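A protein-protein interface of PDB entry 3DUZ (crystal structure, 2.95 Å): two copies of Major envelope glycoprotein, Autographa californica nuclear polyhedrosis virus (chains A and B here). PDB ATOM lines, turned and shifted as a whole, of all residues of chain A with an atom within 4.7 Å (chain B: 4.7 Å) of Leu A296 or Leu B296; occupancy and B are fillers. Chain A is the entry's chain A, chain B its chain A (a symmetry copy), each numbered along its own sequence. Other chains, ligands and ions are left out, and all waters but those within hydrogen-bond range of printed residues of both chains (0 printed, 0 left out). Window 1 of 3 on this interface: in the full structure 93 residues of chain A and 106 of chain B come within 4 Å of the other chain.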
ATOM      1  N   GLU A 292     -29.981 -21.627 -37.271  1.00  0.00           N
ATOM      2  CA  GLU A 292     -29.283 -21.129 -36.090  1.00  0.00           C
ATOM      3  C   GLU A 292     -28.792 -22.259 -35.210  1.00  0.00           C
ATOM      4  O   GLU A 292     -27.677 -22.207 -34.683  1.00  0.00           O
ATOM      5  CB  GLU A 292     -30.169 -20.195 -35.287  1.00  0.00           C
ATOM      6  CG  GLU A 292     -30.209 -18.796 -35.850  1.00  0.00           C
ATOM      7  CD  GLU A 292     -28.909 -18.038 -35.637  1.00  0.00           C
ATOM      8  OE1 GLU A 292     -28.376 -18.052 -34.501  1.00  0.00           O
ATOM      9  OE2 GLU A 292     -28.425 -17.417 -36.609  1.00  0.00           O
ATOM     10  N   ASN A 293     -29.629 -23.282 -35.065  1.00  0.00           N
ATOM     11  CA  ASN A 293     -29.278 -24.445 -34.279  1.00  0.00           C
ATOM     12  C   ASN A 293     -28.057 -25.140 -34.866  1.00  0.00           C
ATOM     13  O   ASN A 293     -27.096 -25.391 -34.149  1.00  0.00           O
ATOM     14  CB  ASN A 293     -30.466 -25.401 -34.181  1.00  0.00           C
ATOM     15  CG  ASN A 293     -30.291 -26.438 -33.088  1.00  0.00           C
ATOM     16  OD1 ASN A 293     -30.157 -27.629 -33.368  1.00  0.00           O
ATOM     17  ND2 ASN A 293     -30.281 -25.990 -31.836  1.00  0.00           N
ATOM     18  N   ASP A 294     -28.086 -25.413 -36.169  1.00  0.00           N
ATOM     19  CA  ASP A 294     -26.949 -26.011 -36.878  1.00  0.00           C
ATOM     20  C   ASP A 294     -25.744 -25.083 -36.945  1.00  0.00           C
ATOM     21  O   ASP A 294     -24.606 -25.547 -37.084  1.00  0.00           O
ATOM     22  CB  ASP A 294     -27.328 -26.402 -38.304  1.00  0.00           C
ATOM     23  CG  ASP A 294     -28.436 -27.425 -38.356  1.00  0.00           C
ATOM     24  OD1 ASP A 294     -28.360 -28.441 -37.640  1.00  0.00           O
ATOM     25  OD2 ASP A 294     -29.387 -27.217 -39.135  1.00  0.00           O
ATOM     26  N   LEU A 295     -25.992 -23.777 -36.879  1.00  0.00           N
ATOM     27  CA  LEU A 295     -24.913 -22.805 -36.851  1.00  0.00           C
ATOM     28  C   LEU A 295     -24.245 -22.834 -35.493  1.00  0.00           C
ATOM     29  O   LEU A 295     -23.028 -22.746 -35.397  1.00  0.00           O
ATOM     30  CB  LEU A 295     -25.434 -21.409 -37.158  1.00  0.00           C
ATOM     31  CG  LEU A 295     -24.390 -20.333 -37.444  1.00  0.00           C
ATOM     32  CD1 LEU A 295     -23.623 -20.622 -38.726  1.00  0.00           C
ATOM     33  CD2 LEU A 295     -25.066 -18.982 -37.527  1.00  0.00           C
ATOM     34  N   LEU A 296     -25.051 -22.971 -34.445  1.00  0.00           N
ATOM     35  CA  LEU A 296     -24.546 -23.124 -33.091  1.00  0.00           C
ATOM     36  C   LEU A 296     -23.672 -24.362 -32.997  1.00  0.00           C
ATOM     37  O   LEU A 296     -22.585 -24.302 -32.426  1.00  0.00           O
ATOM     38  CB  LEU A 296     -25.702 -23.209 -32.093  1.00  0.00           C
ATOM     39  CG  LEU A 296     -25.466 -23.196 -30.571  1.00  0.00           C
ATOM     40  CD1 LEU A 296     -25.298 -24.583 -30.033  1.00  0.00           C
ATOM     41  CD2 LEU A 296     -24.264 -22.364 -30.164  1.00  0.00           C
ATOM     42  N   LYS A 297     -24.140 -25.471 -33.573  1.00  0.00           N
ATOM     43  CA  LYS A 297     -23.432 -26.753 -33.483  1.00  0.00           C
ATOM     44  C   LYS A 297     -22.085 -26.737 -34.199  1.00  0.00           C
ATOM     45  O   LYS A 297     -21.085 -27.204 -33.655  1.00  0.00           O
ATOM     46  CB  LYS A 297     -24.301 -27.903 -34.000  1.00  0.00           C
ATOM     47  CG  LYS A 297     -23.780 -29.287 -33.619  1.00  0.00           C
ATOM     48  CD  LYS A 297     -24.792 -30.405 -33.838  1.00  0.00           C
ATOM     49  CE  LYS A 297     -24.324 -31.653 -33.104  1.00  0.00           C
ATOM     50  NZ  LYS A 297     -25.341 -32.737 -33.152  1.00  0.00           N
ATOM     51  N   MET A 298     -22.066 -26.190 -35.410  1.00  0.00           N
ATOM     52  CA  MET A 298     -20.844 -26.100 -36.198  1.00  0.00           C
ATOM     53  C   MET A 298     -19.789 -25.331 -35.419  1.00  0.00           C
ATOM     54  O   MET A 298     -18.678 -25.820 -35.213  1.00  0.00           O
ATOM     55  CB  MET A 298     -21.114 -25.415 -37.540  1.00  0.00           C
ATOM     56  CG  MET A 298     -19.938 -25.402 -38.489  1.00  0.00           C
ATOM     57  SD  MET A 298     -20.050 -24.040 -39.677  1.00  0.00           S
ATOM     58  CE  MET A 298     -19.166 -22.732 -38.816  1.00  0.00           C
ATOM     59  N   ASN A 299     -20.154 -24.139 -34.963  1.00  0.00           N
ATOM     60  CA  ASN A 299     -19.194 -23.247 -34.330  1.00  0.00           C
ATOM     61  C   ASN A 299     -18.712 -23.733 -32.970  1.00  0.00           C
ATOM     62  O   ASN A 299     -17.521 -23.667 -32.679  1.00  0.00           O
ATOM     63  CB  ASN A 299     -19.741 -21.823 -34.274  1.00  0.00           C
ATOM     64  CG  ASN A 299     -19.601 -21.104 -35.599  1.00  0.00           C
ATOM     65  OD1 ASN A 299     -18.491 -20.811 -36.043  1.00  0.00           O
ATOM     66  ND2 ASN A 299     -20.724 -20.822 -36.244  1.00  0.00           N
ATOM     67  N   ILE A 300     -19.635 -24.242 -32.158  1.00  0.00           N
ATOM     68  CA  ILE A 300     -19.285 -24.893 -30.902  1.00  0.00           C
ATOM     69  C   ILE A 300     -18.286 -26.025 -31.137  1.00  0.00           C
ATOM     70  O   ILE A 300     -17.288 -26.125 -30.426  1.00  0.00           O
ATOM     71  CB  ILE A 300     -20.547 -25.408 -30.161  1.00  0.00           C
ATOM     72  CG1 ILE A 300     -21.208 -24.263 -29.384  1.00  0.00           C
ATOM     73  CG2 ILE A 300     -20.227 -26.586 -29.239  1.00  0.00           C
ATOM     74  CD1 ILE A 300     -20.395 -23.711 -28.217  1.00  0.00           C
ATOM     75  N   ILE A 401     -25.264 -13.360 -21.735  1.00  0.00           N
ATOM     76  CA  ILE A 401     -26.416 -13.994 -22.360  1.00  0.00           C
ATOM     77  C   ILE A 401     -27.607 -13.819 -21.435  1.00  0.00           C
ATOM     78  O   ILE A 401     -27.914 -14.716 -20.654  1.00  0.00           O
ATOM     79  CB  ILE A 401     -26.161 -15.483 -22.626  1.00  0.00           C
ATOM     80  CG1 ILE A 401     -24.887 -15.653 -23.446  1.00  0.00           C
ATOM     81  CG2 ILE A 401     -27.310 -16.097 -23.375  1.00  0.00           C
ATOM     82  CD1 ILE A 401     -24.104 -16.904 -23.121  1.00  0.00           C
ATOM     83  N   GLU B 292     -33.316 -21.763 -27.793  1.00  0.00           N
ATOM     84  CA  GLU B 292     -32.030 -21.516 -28.436  1.00  0.00           C
ATOM     85  C   GLU B 292     -31.135 -20.640 -27.585  1.00  0.00           C
ATOM     86  O   GLU B 292     -29.929 -20.882 -27.485  1.00  0.00           O
ATOM     87  CB  GLU B 292     -32.218 -20.889 -29.805  1.00  0.00           C
ATOM     88  CG  GLU B 292     -32.556 -21.900 -30.872  1.00  0.00           C
ATOM     89  CD  GLU B 292     -31.375 -22.783 -31.240  1.00  0.00           C
ATOM     90  OE1 GLU B 292     -30.261 -22.249 -31.461  1.00  0.00           O
ATOM     91  OE2 GLU B 292     -31.566 -24.016 -31.320  1.00  0.00           O
ATOM     92  N   ASN B 293     -31.739 -19.629 -26.967  1.00  0.00           N
ATOM     93  CA  ASN B 293     -31.013 -18.730 -26.096  1.00  0.00           C
ATOM     94  C   ASN B 293     -30.421 -19.490 -24.916  1.00  0.00           C
ATOM     95  O   ASN B 293     -29.229 -19.377 -24.655  1.00  0.00           O
ATOM     96  CB  ASN B 293     -31.920 -17.595 -25.624  1.00  0.00           C
ATOM     97  CG  ASN B 293     -31.144 -16.440 -25.022  1.00  0.00           C
ATOM     98  OD1 ASN B 293     -31.240 -16.176 -23.823  1.00  0.00           O
ATOM     99  ND2 ASN B 293     -30.362 -15.751 -25.848  1.00  0.00           N
ATOM    100  N   ASP B 294     -31.245 -20.283 -24.234  1.00  0.00           N
ATOM    101  CA  ASP B 294     -30.791 -21.128 -23.124  1.00  0.00           C
ATOM    102  C   ASP B 294     -29.852 -22.239 -23.576  1.00  0.00           C
ATOM    103  O   ASP B 294     -29.047 -22.738 -22.780  1.00  0.00           O
ATOM    104  CB  ASP B 294     -31.971 -21.771 -22.398  1.00  0.00           C
ATOM    105  CG  ASP B 294     -32.908 -20.756 -21.793  1.00  0.00           C
ATOM    106  OD1 ASP B 294     -32.439 -19.827 -21.109  1.00  0.00           O
ATOM    107  OD2 ASP B 294     -34.131 -20.898 -21.990  1.00  0.00           O
ATOM    108  N   LEU B 295     -29.973 -22.647 -24.837  1.00  0.00           N
ATOM    109  CA  LEU B 295     -29.074 -23.641 -25.397  1.00  0.00           C
ATOM    110  C   LEU B 295     -27.719 -23.014 -25.641  1.00  0.00           C
ATOM    111  O   LEU B 295     -26.693 -23.635 -25.395  1.00  0.00           O
ATOM    112  CB  LEU B 295     -29.637 -24.210 -26.691  1.00  0.00           C
ATOM    113  CG  LEU B 295     -28.954 -25.458 -27.247  1.00  0.00           C
ATOM    114  CD1 LEU B 295     -29.135 -26.654 -26.325  1.00  0.00           C
ATOM    115  CD2 LEU B 295     -29.505 -25.765 -28.623  1.00  0.00           C
ATOM    116  N   LEU B 296     -27.724 -21.771 -26.114  1.00  0.00           N
ATOM    117  CA  LEU B 296     -26.502 -21.004 -26.293  1.00  0.00           C
ATOM    118  C   LEU B 296     -25.786 -20.845 -24.964  1.00  0.00           C
ATOM    119  O   LEU B 296     -24.575 -21.044 -24.894  1.00  0.00           O
ATOM    120  CB  LEU B 296     -26.814 -19.634 -26.899  1.00  0.00           C
ATOM    121  CG  LEU B 296     -25.699 -18.677 -27.362  1.00  0.00           C
ATOM    122  CD1 LEU B 296     -25.276 -17.757 -26.260  1.00  0.00           C
ATOM    123  CD2 LEU B 296     -24.476 -19.402 -27.891  1.00  0.00           C
ATOM    124  N   LYS B 297     -26.537 -20.509 -23.914  1.00  0.00           N
ATOM    125  CA  LYS B 297     -25.956 -20.245 -22.594  1.00  0.00           C
ATOM    126  C   LYS B 297     -25.323 -21.485 -21.968  1.00  0.00           C
ATOM    127  O   LYS B 297     -24.212 -21.419 -21.443  1.00  0.00           O
ATOM    128  CB  LYS B 297     -26.991 -19.633 -21.644  1.00  0.00           C
ATOM    129  CG  LYS B 297     -26.382 -19.016 -20.387  1.00  0.00           C
ATOM    130  CD  LYS B 297     -27.348 -18.128 -19.610  1.00  0.00           C
ATOM    131  CE  LYS B 297     -26.564 -17.292 -18.612  1.00  0.00           C
ATOM    132  NZ  LYS B 297     -27.428 -16.294 -17.927  1.00  0.00           N
ATOM    133  N   MET B 298     -26.031 -22.607 -22.035  1.00  0.00           N
ATOM    134  CA  MET B 298     -25.540 -23.865 -21.487  1.00  0.00           C
ATOM    135  C   MET B 298     -24.208 -24.217 -22.130  1.00  0.00           C
ATOM    136  O   MET B 298     -23.215 -24.444 -21.438  1.00  0.00           O
ATOM    137  CB  MET B 298     -26.554 -24.989 -21.718  1.00  0.00           C
ATOM    138  CG  MET B 298     -26.199 -26.302 -21.059  1.00  0.00           C
ATOM    139  SD  MET B 298     -26.973 -27.705 -21.900  1.00  0.00           S
ATOM    140  CE  MET B 298     -25.713 -28.151 -23.104  1.00  0.00           C
ATOM    141  N   ASN B 299     -24.189 -24.233 -23.457  1.00  0.00           N
ATOM    142  CA  ASN B 299     -23.017 -24.694 -24.189  1.00  0.00           C
ATOM    143  C   ASN B 299     -21.820 -23.759 -24.079  1.00  0.00           C
ATOM    144  O   ASN B 299     -20.697 -24.218 -23.889  1.00  0.00           O
ATOM    145  CB  ASN B 299     -23.379 -25.003 -25.639  1.00  0.00           C
ATOM    146  CG  ASN B 299     -24.055 -26.349 -25.785  1.00  0.00           C
ATOM    147  OD1 ASN B 299     -23.438 -27.392 -25.569  1.00  0.00           O
ATOM    148  ND2 ASN B 299     -25.331 -26.338 -26.147  1.00  0.00           N
ATOM    149  N   ILE B 300     -22.071 -22.457 -24.175  1.00  0.00           N
ATOM    150  CA  ILE B 300     -21.047 -21.452 -23.920  1.00  0.00           C
ATOM    151  C   ILE B 300     -20.428 -21.645 -22.537  1.00  0.00           C
ATOM    152  O   ILE B 300     -19.207 -21.624 -22.397  1.00  0.00           O
ATOM    153  CB  ILE B 300     -21.609 -20.016 -24.084  1.00  0.00           C
ATOM    154  CG1 ILE B 300     -21.629 -19.622 -25.567  1.00  0.00           C
ATOM    155  CG2 ILE B 300     -20.826 -18.997 -23.255  1.00  0.00           C
ATOM    156  CD1 ILE B 300     -20.259 -19.470 -26.221  1.00  0.00           C
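Of the 10 printed residues of chain A, 3 touch a printed residue of chain B. Printed residues of chain A that touch a printed residue of chain B: Asn A293, Leu A296 and Ile A401. Among the printed residues, no Asp or Glu carboxylate lies within 4 Å of a Lys or Arg side-chain nitrogen of the other chain.
ND2 of Asn A293 is in hydrogen-bond range of OE2 of Glu B292 (2.4 Å). The backbone carbonyl oxygen (O) of Ile A401 sits at hydrogen-bond distance from the side-chain amino group (NZ) of Lys B297 (3.2 Å).
The backbone carbonyl oxygen (O) of Leu B295 is in hydrogen-bond range of the side-chain amide nitrogen (ND2) of Asn B299 (3.1 Å).
Printed residues of chain B within 4 Å of Leu A296: Leu B296 (3.7 Å). Of chain A, only Leu A296 (3.7 Å) and Ile A401 (3.5 Å) come within 4 Å of Leu B296. Of the printed residues of chain B, Asn A293 touches Glu B292 (2.4 Å) and Leu B295 (3.3 Å). Printed residues of chain A within 4 Å of Lys B297: Ile A401. Of the printed residues of chain B, Ile A401 touches Asn B293, Leu B296, Lys B297 and Ile B300. Of the printed residues of chain A, Glu B292 touches Asn A293. Of the printed residues of chain A, Asn B293 touches Ile A401. Asn A299 touches none of the printed residues of chain B. Leu A295 touches none of the printed residues of chain B. The nearest printed residue of chain A that does not touch Leu B296 is Ile A300 (5.9 Å).
Among the printed residues, merely in contact across the chains: Asn A293 with Leu B295 (3.3 Å), Ile A401 with Leu B296 (3.5 Å), Leu A296 with Leu B296 (3.7 Å), Ile A401 with Ile B300 (3.9 Å) and Ile A401 with Asn B293 (3.9 Å).
Asn A293 touches Glu B292, but with the chains exchanged Glu A292 does not touch Asn B293 (8.4 Å). Asn A293 touches Leu B295, but with the chains exchanged Leu A295 does not touch Asn B293 (11.8 Å). Leu B296 touches its own counterpart, Leu A296.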
